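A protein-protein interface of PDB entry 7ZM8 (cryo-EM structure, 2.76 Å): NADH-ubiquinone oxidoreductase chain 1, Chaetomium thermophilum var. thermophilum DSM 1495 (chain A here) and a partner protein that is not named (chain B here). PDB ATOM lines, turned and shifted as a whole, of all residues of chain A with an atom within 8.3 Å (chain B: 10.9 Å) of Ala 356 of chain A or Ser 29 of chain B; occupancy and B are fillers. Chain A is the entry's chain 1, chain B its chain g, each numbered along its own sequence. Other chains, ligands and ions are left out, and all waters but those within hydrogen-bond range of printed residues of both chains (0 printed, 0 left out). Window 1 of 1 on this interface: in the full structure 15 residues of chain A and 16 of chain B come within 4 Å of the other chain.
O of Gly 36 of chain B sits close to SG of Cys 363 of chain A (3.7 Å).
The backbone carbonyl oxygen of Val 359 of chain A sits at hydrogen-bond distance from the side-chain sulfur of Cys 363 of chain A (3.3 Å). The backbone carbonyl oxygen (O) of Ala 25 of chain B sits at hydrogen-bond distance from the side-chain hydroxyl (OG) of Ser 29 of chain B (2.5 Å).
Among the printed residues, pairs that only touch across the chains: Thr 348 of chain A with Leu 26 of chain B (3.9 Å), Val 349 of chain A with Ala 25 of chain B (3.7 Å), Pro 352 of chain A with Ser 29 of chain B (3.4 Å), Ile 353 of chain A with Ala 25 of chain B (3.4 Å), Ile 353 of chain A with Ser 29 of chain B (3.1 Å), Ala 356 of chain A with Ser 29 of chain B (3.2 Å), Ala 356 of chain A with Ile 32 of chain B (3.6 Å), Ala 356 of chain A with Gly 33 of chain B (3.9 Å), Leu 357 of chain A with Ile 32 of chain B (3.9 Å), Val 359 of chain A with Gly 33 of chain B (3.9 Å), Leu 360 of chain A with Ile 32 of chain B (3.8 Å), Leu 360 of chain A with Leu 35 of chain B (3.7 Å), Leu 360 of chain A with Gly 36 of chain B (3.6 Å) and Cys 363 of chain A with Thr 39 of chain B (3.9 Å).
Ala 356 of chain A touches just these residues of chain B: Ser 29 (3.2 Å), Ile 32 (3.6 Å) and Gly 33 (3.9 Å). Ser 29 of chain B touches three residues of chain A. Of chain B, only Ala 25 (3.4 Å) and Ser 29 (3.1 Å) come within 4 Å of Ile 353 of chain A. Val 359 of chain A touches just one residue of chain B: Gly 33. Leu 360 of chain A touches just these residues of chain B: Ile 32, Leu 35 and Gly 36. Of the printed residues of chain B, Thr 348 of chain A touches Leu 26 (3.9 Å). Of the printed residues of chain B, Val 349 of chain A touches Ala 25 (3.7 Å). Of the printed residues of chain A, Leu 35 of chain B touches Leu 360 (3.7 Å). Printed residues of chain B within 4 Å of Cys 363 of chain A: Gly 36 (3.6 Å) and Thr 39 (3.9 Å). The nearest residue of chain A that does not touch Ser 29 of chain B is Val 349 of chain A (5.0 Å). The nearest printed residue of chain A that does not touch Gly 33 of chain B is Leu 360 of chain A (5.8 Å).
Of the 19 printed residues of chain B, 8 touch a printed residue of chain A. Printed residues of chain A that touch a printed residue of chain B: Thr 348, Val 349, Pro 352, Ile 353, Ala 356, Leu 357, Val 359, Leu 360 and Cys 363. Hydrophobic or aromatic side chains of chain A within 4 Å of the printed part of chain B: Val 349, Pro 352, Ile 353, Ala 356, Leu 357, Val 359 and Leu 360. Among the printed residues, 15 pairs touch across the chains.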
ATOM      1  N   LEU A 161     -13.281 -20.650  -7.720  1.00  0.00           N
ATOM      2  CA  LEU A 161     -13.216 -20.315  -6.304  1.00  0.00           C
ATOM      3  C   LEU A 161     -14.157 -19.173  -5.946  1.00  0.00           C
ATOM      4  O   LEU A 161     -14.595 -19.073  -4.798  1.00  0.00           O
ATOM      5  CB  LEU A 161     -11.777 -19.973  -5.925  1.00  0.00           C
ATOM      6  CG  LEU A 161     -10.837 -21.175  -5.900  1.00  0.00           C
ATOM      7  CD1 LEU A 161      -9.415 -20.761  -6.211  1.00  0.00           C
ATOM      8  CD2 LEU A 161     -10.914 -21.880  -4.560  1.00  0.00           C
ATOM      9  N   THR A 348       3.949 -25.459 -12.666  1.00  0.00           N
ATOM     10  CA  THR A 348       4.669 -25.888 -11.480  1.00  0.00           C
ATOM     11  C   THR A 348       4.571 -24.900 -10.329  1.00  0.00           C
ATOM     12  O   THR A 348       5.070 -25.193  -9.240  1.00  0.00           O
ATOM     13  CB  THR A 348       6.140 -26.148 -11.818  1.00  0.00           C
ATOM     14  OG1 THR A 348       6.816 -24.906 -12.027  1.00  0.00           O
ATOM     15  CG2 THR A 348       6.248 -26.991 -13.071  1.00  0.00           C
ATOM     16  N   VAL A 349       3.937 -23.753 -10.548  1.00  0.00           N
ATOM     17  CA  VAL A 349       3.773 -22.776  -9.431  1.00  0.00           C
ATOM     18  C   VAL A 349       2.314 -22.389  -9.193  1.00  0.00           C
ATOM     19  O   VAL A 349       1.853 -22.603  -8.079  1.00  0.00           O
ATOM     20  CB  VAL A 349       4.668 -21.524  -9.588  1.00  0.00           C
ATOM     21  CG1 VAL A 349       4.326 -20.442  -8.577  1.00  0.00           C
ATOM     22  CG2 VAL A 349       6.150 -21.851  -9.553  1.00  0.00           C
ATOM     23  N   LEU A 350       1.577 -21.962 -10.205  1.00  0.00           N
ATOM     24  CA  LEU A 350       0.220 -21.386  -9.997  1.00  0.00           C
ATOM     25  C   LEU A 350      -0.867 -22.447 -10.025  1.00  0.00           C
ATOM     26  O   LEU A 350      -1.796 -22.315  -9.234  1.00  0.00           O
ATOM     27  CB  LEU A 350      -0.068 -20.351 -11.090  1.00  0.00           C
ATOM     28  CG  LEU A 350       0.792 -19.093 -11.132  1.00  0.00           C
ATOM     29  CD1 LEU A 350       0.375 -18.241 -12.315  1.00  0.00           C
ATOM     30  CD2 LEU A 350       0.658 -18.303  -9.842  1.00  0.00           C
ATOM     31  N   LEU A 351      -0.755 -23.467 -10.857  1.00  0.00           N
ATOM     32  CA  LEU A 351      -1.765 -24.520 -10.785  1.00  0.00           C
ATOM     33  C   LEU A 351      -1.706 -25.352  -9.511  1.00  0.00           C
ATOM     34  O   LEU A 351      -2.779 -25.692  -8.990  1.00  0.00           O
ATOM     35  CB  LEU A 351      -1.671 -25.417 -12.023  1.00  0.00           C
ATOM     36  CG  LEU A 351      -2.416 -24.889 -13.243  1.00  0.00           C
ATOM     37  CD1 LEU A 351      -2.297 -25.869 -14.375  1.00  0.00           C
ATOM     38  CD2 LEU A 351      -3.874 -24.615 -12.909  1.00  0.00           C
ATOM     39  N   PRO A 352      -0.540 -25.757  -8.993  1.00  0.00           N
ATOM     40  CA  PRO A 352      -0.542 -26.444  -7.693  1.00  0.00           C
ATOM     41  C   PRO A 352      -1.138 -25.619  -6.566  1.00  0.00           C
ATOM     42  O   PRO A 352      -1.829 -26.168  -5.704  1.00  0.00           O
ATOM     43  CB  PRO A 352       0.945 -26.739  -7.461  1.00  0.00           C
ATOM     44  CG  PRO A 352       1.506 -26.830  -8.805  1.00  0.00           C
ATOM     45  CD  PRO A 352       0.793 -25.808  -9.615  1.00  0.00           C
ATOM     46  N   ILE A 353      -0.883 -24.311  -6.546  1.00  0.00           N
ATOM     47  CA  ILE A 353      -1.452 -23.462  -5.507  1.00  0.00           C
ATOM     48  C   ILE A 353      -2.964 -23.390  -5.649  1.00  0.00           C
ATOM     49  O   ILE A 353      -3.697 -23.459  -4.658  1.00  0.00           O
ATOM     50  CB  ILE A 353      -0.808 -22.063  -5.544  1.00  0.00           C
ATOM     51  CG1 ILE A 353       0.678 -22.149  -5.205  1.00  0.00           C
ATOM     52  CG2 ILE A 353      -1.507 -21.125  -4.577  1.00  0.00           C
ATOM     53  CD1 ILE A 353       0.952 -22.645  -3.803  1.00  0.00           C
ATOM     54  N   LEU A 354      -3.451 -23.243  -6.879  1.00  0.00           N
ATOM     55  CA  LEU A 354      -4.889 -23.186  -7.109  1.00  0.00           C
ATOM     56  C   LEU A 354      -5.572 -24.482  -6.697  1.00  0.00           C
ATOM     57  O   LEU A 354      -6.635 -24.459  -6.069  1.00  0.00           O
ATOM     58  CB  LEU A 354      -5.165 -22.885  -8.581  1.00  0.00           C
ATOM     59  CG  LEU A 354      -5.163 -21.420  -8.996  1.00  0.00           C
ATOM     60  CD1 LEU A 354      -5.393 -21.309 -10.487  1.00  0.00           C
ATOM     61  CD2 LEU A 354      -6.214 -20.647  -8.229  1.00  0.00           C
ATOM     62  N   PHE A 355      -4.976 -25.623  -7.040  1.00  0.00           N
ATOM     63  CA  PHE A 355      -5.568 -26.906  -6.682  1.00  0.00           C
ATOM     64  C   PHE A 355      -5.600 -27.095  -5.172  1.00  0.00           C
ATOM     65  O   PHE A 355      -6.549 -27.675  -4.632  1.00  0.00           O
ATOM     66  CB  PHE A 355      -4.796 -28.037  -7.353  1.00  0.00           C
ATOM     67  CG  PHE A 355      -4.949 -28.078  -8.846  1.00  0.00           C
ATOM     68  CD1 PHE A 355      -5.915 -27.311  -9.483  1.00  0.00           C
ATOM     69  CD2 PHE A 355      -4.116 -28.866  -9.615  1.00  0.00           C
ATOM     70  CE1 PHE A 355      -6.053 -27.338 -10.852  1.00  0.00           C
ATOM     71  CE2 PHE A 355      -4.247 -28.896 -10.987  1.00  0.00           C
ATOM     72  CZ  PHE A 355      -5.218 -28.132 -11.606  1.00  0.00           C
ATOM     73  N   ALA A 356      -4.562 -26.630  -4.477  1.00  0.00           N
ATOM     74  CA  ALA A 356      -4.562 -26.665  -3.021  1.00  0.00           C
ATOM     75  C   ALA A 356      -5.645 -25.766  -2.449  1.00  0.00           C
ATOM     76  O   ALA A 356      -6.276 -26.102  -1.441  1.00  0.00           O
ATOM     77  CB  ALA A 356      -3.193 -26.253  -2.494  1.00  0.00           C
ATOM     78  N   LEU A 357      -5.859 -24.603  -3.066  1.00  0.00           N
ATOM     79  CA  LEU A 357      -6.924 -23.713  -2.624  1.00  0.00           C
ATOM     80  C   LEU A 357      -8.290 -24.243  -3.026  1.00  0.00           C
ATOM     81  O   LEU A 357      -9.286 -23.943  -2.362  1.00  0.00           O
ATOM     82  CB  LEU A 357      -6.705 -22.315  -3.193  1.00  0.00           C
ATOM     83  CG  LEU A 357      -5.620 -21.476  -2.521  1.00  0.00           C
ATOM     84  CD1 LEU A 357      -5.510 -20.128  -3.199  1.00  0.00           C
ATOM     85  CD2 LEU A 357      -5.903 -21.319  -1.044  1.00  0.00           C
ATOM     86  N   ILE A 358      -8.353 -25.023  -4.104  1.00  0.00           N
ATOM     87  CA  ILE A 358      -9.600 -25.665  -4.505  1.00  0.00           C
ATOM     88  C   ILE A 358     -10.042 -26.660  -3.444  1.00  0.00           C
ATOM     89  O   ILE A 358     -11.239 -26.849  -3.211  1.00  0.00           O
ATOM     90  CB  ILE A 358      -9.432 -26.329  -5.887  1.00  0.00           C
ATOM     91  CG1 ILE A 358      -9.584 -25.294  -7.004  1.00  0.00           C
ATOM     92  CG2 ILE A 358     -10.408 -27.478  -6.079  1.00  0.00           C
ATOM     93  CD1 ILE A 358      -9.154 -25.796  -8.365  1.00  0.00           C
ATOM     94  N   VAL A 359      -9.084 -27.322  -2.798  1.00  0.00           N
ATOM     95  CA  VAL A 359      -9.407 -28.200  -1.679  1.00  0.00           C
ATOM     96  C   VAL A 359      -9.824 -27.384  -0.463  1.00  0.00           C
ATOM     97  O   VAL A 359     -10.872 -27.629   0.142  1.00  0.00           O
ATOM     98  CB  VAL A 359      -8.207 -29.106  -1.354  1.00  0.00           C
ATOM     99  CG1 VAL A 359      -8.307 -29.636   0.061  1.00  0.00           C
ATOM    100  CG2 VAL A 359      -8.131 -30.239  -2.332  1.00  0.00           C
ATOM    101  N   LEU A 360      -9.020 -26.381  -0.113  1.00  0.00           N
ATOM    102  CA  LEU A 360      -9.153 -25.698   1.169  1.00  0.00           C
ATOM    103  C   LEU A 360     -10.458 -24.917   1.275  1.00  0.00           C
ATOM    104  O   LEU A 360     -11.132 -24.959   2.307  1.00  0.00           O
ATOM    105  CB  LEU A 360      -7.959 -24.766   1.367  1.00  0.00           C
ATOM    106  CG  LEU A 360      -7.912 -23.921   2.637  1.00  0.00           C
ATOM    107  CD1 LEU A 360      -7.446 -24.737   3.825  1.00  0.00           C
ATOM    108  CD2 LEU A 360      -7.034 -22.711   2.422  1.00  0.00           C
ATOM    109  N   VAL A 361     -10.823 -24.183   0.225  1.00  0.00           N
ATOM    110  CA  VAL A 361     -11.918 -23.218   0.341  1.00  0.00           C
ATOM    111  C   VAL A 361     -13.256 -23.876   0.657  1.00  0.00           C
ATOM    112  O   VAL A 361     -13.947 -23.406   1.574  1.00  0.00           O
ATOM    113  CB  VAL A 361     -11.968 -22.324  -0.911  1.00  0.00           C
ATOM    114  CG1 VAL A 361     -13.305 -21.630  -1.022  1.00  0.00           C
ATOM    115  CG2 VAL A 361     -10.855 -21.303  -0.854  1.00  0.00           C
ATOM    116  N   PRO A 362     -13.693 -24.928  -0.044  1.00  0.00           N
ATOM    117  CA  PRO A 362     -14.926 -25.604   0.383  1.00  0.00           C
ATOM    118  C   PRO A 362     -14.824 -26.225   1.762  1.00  0.00           C
ATOM    119  O   PRO A 362     -15.840 -26.348   2.451  1.00  0.00           O
ATOM    120  CB  PRO A 362     -15.138 -26.664  -0.706  1.00  0.00           C
ATOM    121  CG  PRO A 362     -13.826 -26.870  -1.294  1.00  0.00           C
ATOM    122  CD  PRO A 362     -13.160 -25.541  -1.271  1.00  0.00           C
ATOM    123  N   CYS A 363     -13.629 -26.635   2.180  1.00  0.00           N
ATOM    124  CA  CYS A 363     -13.469 -27.210   3.510  1.00  0.00           C
ATOM    125  C   CYS A 363     -13.707 -26.169   4.595  1.00  0.00           C
ATOM    126  O   CYS A 363     -14.284 -26.478   5.641  1.00  0.00           O
ATOM    127  CB  CYS A 363     -12.082 -27.833   3.641  1.00  0.00           C
ATOM    128  SG  CYS A 363     -11.883 -29.388   2.759  1.00  0.00           S
ATOM    129  N   ALA B  19      12.676 -27.737   1.611  1.00  0.00           N
ATOM    130  CA  ALA B  19      11.594 -27.590   0.645  1.00  0.00           C
ATOM    131  C   ALA B  19      10.864 -26.271   0.836  1.00  0.00           C
ATOM    132  O   ALA B  19      10.446 -25.641  -0.139  1.00  0.00           O
ATOM    133  CB  ALA B  19      10.623 -28.766   0.757  1.00  0.00           C
ATOM    134  N   ALA B  20      10.694 -25.840   2.084  1.00  0.00           N
ATOM    135  CA  ALA B  20      10.090 -24.537   2.329  1.00  0.00           C
ATOM    136  C   ALA B  20      10.939 -23.414   1.752  1.00  0.00           C
ATOM    137  O   ALA B  20      10.401 -22.384   1.330  1.00  0.00           O
ATOM    138  CB  ALA B  20       9.877 -24.330   3.826  1.00  0.00           C
ATOM    139  N   ARG B  23      11.785 -25.157  -2.625  1.00  0.00           N
ATOM    140  CA  ARG B  23      10.631 -25.484  -3.462  1.00  0.00           C
ATOM    141  C   ARG B  23       9.376 -24.889  -2.838  1.00  0.00           C
ATOM    142  O   ARG B  23       8.455 -25.612  -2.454  1.00  0.00           O
ATOM    143  CB  ARG B  23      10.496 -26.997  -3.620  1.00  0.00           C
ATOM    144  CG  ARG B  23      11.762 -27.683  -4.068  1.00  0.00           C
ATOM    145  CD  ARG B  23      11.969 -27.525  -5.557  1.00  0.00           C
ATOM    146  NE  ARG B  23      13.141 -28.260  -6.010  1.00  0.00           N
ATOM    147  CZ  ARG B  23      14.387 -27.819  -5.904  1.00  0.00           C
ATOM    148  NH1 ARG B  23      14.630 -26.633  -5.364  1.00  0.00           N
ATOM    149  NH2 ARG B  23      15.393 -28.560  -6.343  1.00  0.00           N
ATOM    150  N   PRO B  24       9.304 -23.559  -2.734  1.00  0.00           N
ATOM    151  CA  PRO B  24       8.232 -22.961  -1.924  1.00  0.00           C
ATOM    152  C   PRO B  24       6.843 -23.152  -2.503  1.00  0.00           C
ATOM    153  O   PRO B  24       5.910 -23.439  -1.749  1.00  0.00           O
ATOM    154  CB  PRO B  24       8.623 -21.478  -1.852  1.00  0.00           C
ATOM    155  CG  PRO B  24       9.751 -21.288  -2.767  1.00  0.00           C
ATOM    156  CD  PRO B  24      10.134 -22.553  -3.411  1.00  0.00           C
ATOM    157  N   ALA B  25       6.673 -23.002  -3.817  1.00  0.00           N
ATOM    158  CA  ALA B  25       5.343 -23.144  -4.403  1.00  0.00           C
ATOM    159  C   ALA B  25       4.807 -24.554  -4.213  1.00  0.00           C
ATOM    160  O   ALA B  25       3.630 -24.741  -3.889  1.00  0.00           O
ATOM    161  CB  ALA B  25       5.371 -22.781  -5.885  1.00  0.00           C
ATOM    162  N   LEU B  26       5.659 -25.559  -4.416  1.00  0.00           N
ATOM    163  CA  LEU B  26       5.234 -26.937  -4.219  1.00  0.00           C
ATOM    164  C   LEU B  26       5.012 -27.250  -2.749  1.00  0.00           C
ATOM    165  O   LEU B  26       4.031 -27.912  -2.396  1.00  0.00           O
ATOM    166  CB  LEU B  26       6.266 -27.897  -4.807  1.00  0.00           C
ATOM    167  CG  LEU B  26       6.220 -28.107  -6.316  1.00  0.00           C
ATOM    168  CD1 LEU B  26       7.026 -29.332  -6.686  1.00  0.00           C
ATOM    169  CD2 LEU B  26       4.789 -28.231  -6.796  1.00  0.00           C
ATOM    170  N   PHE B  27       5.919 -26.804  -1.880  1.00  0.00           N
ATOM    171  CA  PHE B  27       5.825 -27.171  -0.472  1.00  0.00           C
ATOM    172  C   PHE B  27       4.539 -26.646   0.146  1.00  0.00           C
ATOM    173  O   PHE B  27       3.843 -27.367   0.869  1.00  0.00           O
ATOM    174  CB  PHE B  27       7.037 -26.656   0.300  1.00  0.00           C
ATOM    175  CG  PHE B  27       6.939 -26.883   1.777  1.00  0.00           C
ATOM    176  CD1 PHE B  27       7.153 -28.142   2.308  1.00  0.00           C
ATOM    177  CD2 PHE B  27       6.606 -25.847   2.635  1.00  0.00           C
ATOM    178  CE1 PHE B  27       7.049 -28.358   3.654  1.00  0.00           C
ATOM    179  CE2 PHE B  27       6.503 -26.059   3.984  1.00  0.00           C
ATOM    180  CZ  PHE B  27       6.723 -27.316   4.495  1.00  0.00           C
ATOM    181  N   PHE B  28       4.194 -25.400  -0.144  1.00  0.00           N
ATOM    182  CA  PHE B  28       3.012 -24.803   0.452  1.00  0.00           C
ATOM    183  C   PHE B  28       1.727 -25.201  -0.258  1.00  0.00           C
ATOM    184  O   PHE B  28       0.648 -25.006   0.301  1.00  0.00           O
ATOM    185  CB  PHE B  28       3.184 -23.288   0.503  1.00  0.00           C
ATOM    186  CG  PHE B  28       4.260 -22.854   1.455  1.00  0.00           C
ATOM    187  CD1 PHE B  28       4.065 -22.941   2.821  1.00  0.00           C
ATOM    188  CD2 PHE B  28       5.480 -22.403   0.994  1.00  0.00           C
ATOM    189  CE1 PHE B  28       5.055 -22.561   3.699  1.00  0.00           C
ATOM    190  CE2 PHE B  28       6.469 -22.027   1.865  1.00  0.00           C
ATOM    191  CZ  PHE B  28       6.255 -22.104   3.218  1.00  0.00           C
ATOM    192  N   SER B  29       1.814 -25.838  -1.406  1.00  0.00           N
ATOM    193  CA  SER B  29       0.593 -26.397  -2.020  1.00  0.00           C
ATOM    194  C   SER B  29       0.240 -27.603  -1.162  1.00  0.00           C
ATOM    195  O   SER B  29      -0.927 -27.761  -0.800  1.00  0.00           O
ATOM    196  CB  SER B  29       0.851 -26.824  -3.419  1.00  0.00           C
ATOM    197  OG  SER B  29       1.309 -25.746  -4.203  1.00  0.00           O
ATOM    198  N   VAL B  30       1.232 -28.435  -0.874  1.00  0.00           N
ATOM    199  CA  VAL B  30       1.009 -29.652  -0.052  1.00  0.00           C
ATOM    200  C   VAL B  30       0.533 -29.223   1.334  1.00  0.00           C
ATOM    201  O   VAL B  30      -0.331 -29.904   1.891  1.00  0.00           O
ATOM    202  CB  VAL B  30       2.283 -30.519  -0.015  1.00  0.00           C
ATOM    203  CG1 VAL B  30       2.121 -31.751   0.861  1.00  0.00           C
ATOM    204  CG2 VAL B  30       2.728 -30.917  -1.411  1.00  0.00           C
ATOM    205  N   VAL B  31       1.066 -28.125   1.852  1.00  0.00           N
ATOM    206  CA  VAL B  31       0.687 -27.603   3.194  1.00  0.00           C
ATOM    207  C   VAL B  31      -0.736 -27.039   3.151  1.00  0.00           C
ATOM    208  O   VAL B  31      -1.518 -27.421   4.017  1.00  0.00           O
ATOM    209  CB  VAL B  31       1.725 -26.575   3.690  1.00  0.00           C
ATOM    210  CG1 VAL B  31       1.208 -25.735   4.846  1.00  0.00           C
ATOM    211  CG2 VAL B  31       3.028 -27.249   4.068  1.00  0.00           C
ATOM    212  N   ILE B  32      -1.061 -26.183   2.176  1.00  0.00           N
ATOM    213  CA  ILE B  32      -2.417 -25.650   2.085  1.00  0.00           C
ATOM    214  C   ILE B  32      -3.414 -26.775   1.857  1.00  0.00           C
ATOM    215  O   ILE B  32      -4.521 -26.767   2.407  1.00  0.00           O
ATOM    216  CB  ILE B  32      -2.511 -24.580   0.982  1.00  0.00           C
ATOM    217  CG1 ILE B  32      -1.765 -23.314   1.397  1.00  0.00           C
ATOM    218  CG2 ILE B  32      -3.963 -24.256   0.666  1.00  0.00           C
ATOM    219  CD1 ILE B  32      -1.290 -22.488   0.227  1.00  0.00           C
ATOM    220  N   GLY B  33      -3.034 -27.768   1.059  1.00  0.00           N
ATOM    221  CA  GLY B  33      -3.900 -28.918   0.879  1.00  0.00           C
ATOM    222  C   GLY B  33      -4.167 -29.658   2.175  1.00  0.00           C
ATOM    223  O   GLY B  33      -5.292 -30.092   2.431  1.00  0.00           O
ATOM    224  N   ALA B  34      -3.137 -29.812   3.009  1.00  0.00           N
ATOM    225  CA  ALA B  34      -3.318 -30.502   4.280  1.00  0.00           C
ATOM    226  C   ALA B  34      -4.131 -29.673   5.267  1.00  0.00           C
ATOM    227  O   ALA B  34      -4.802 -30.231   6.138  1.00  0.00           O
ATOM    228  CB  ALA B  34      -1.961 -30.859   4.880  1.00  0.00           C
ATOM    229  N   LEU B  35      -4.086 -28.346   5.150  1.00  0.00           N
ATOM    230  CA  LEU B  35      -4.879 -27.496   6.028  1.00  0.00           C
ATOM    231  C   LEU B  35      -6.373 -27.631   5.779  1.00  0.00           C
ATOM    232  O   LEU B  35      -7.164 -27.229   6.634  1.00  0.00           O
ATOM    233  CB  LEU B  35      -4.459 -26.037   5.870  1.00  0.00           C
ATOM    234  CG  LEU B  35      -3.042 -25.717   6.336  1.00  0.00           C
ATOM    235  CD1 LEU B  35      -2.681 -24.280   6.006  1.00  0.00           C
ATOM    236  CD2 LEU B  35      -2.913 -25.978   7.826  1.00  0.00           C
ATOM    237  N   GLY B  36      -6.777 -28.166   4.632  1.00  0.00           N
ATOM    238  CA  GLY B  36      -8.169 -28.422   4.361  1.00  0.00           C
ATOM    239  C   GLY B  36      -8.697 -29.582   5.178  1.00  0.00           C
ATOM    240  O   GLY B  36      -9.768 -29.514   5.785  1.00  0.00           O
ATOM    241  N   PRO B  37      -8.002 -30.731   5.201  1.00  0.00           N
ATOM    242  CA  PRO B  37      -8.469 -31.782   6.095  1.00  0.00           C
ATOM    243  C   PRO B  37      -8.311 -31.423   7.577  1.00  0.00           C
ATOM    244  O   PRO B  37      -9.073 -31.951   8.343  1.00  0.00           O
ATOM    245  CB  PRO B  37      -7.426 -32.845   5.773  1.00  0.00           C
ATOM    246  CG  PRO B  37      -6.958 -32.468   4.391  1.00  0.00           C
ATOM    247  N   VAL B  38      -7.373 -30.529   7.935  1.00  0.00           N
ATOM    248  CA  VAL B  38      -7.267 -30.114   9.330  1.00  0.00           C
ATOM    249  C   VAL B  38      -8.451 -29.244   9.731  1.00  0.00           C
ATOM    250  O   VAL B  38      -9.032 -29.428  10.805  1.00  0.00           O
ATOM    251  CB  VAL B  38      -5.933 -29.388   9.573  1.00  0.00           C
ATOM    252  CG1 VAL B  38      -5.874 -28.863  10.994  1.00  0.00           C
ATOM    253  CG2 VAL B  38      -4.776 -30.323   9.326  1.00  0.00           C
ATOM    254  N   THR B  39      -8.825 -28.278   8.885  1.00  0.00           N
ATOM    255  CA  THR B  39      -9.894 -27.363   9.275  1.00  0.00           C
ATOM    256  C   THR B  39     -11.218 -28.095   9.417  1.00  0.00           C
ATOM    257  O   THR B  39     -12.061 -27.695  10.226  1.00  0.00           O
ATOM    258  CB  THR B  39     -10.022 -26.202   8.275  1.00  0.00           C
ATOM    259  OG1 THR B  39     -11.128 -25.370   8.638  1.00  0.00           O
ATOM    260  CG2 THR B  39     -10.266 -26.700   6.878  1.00  0.00           C
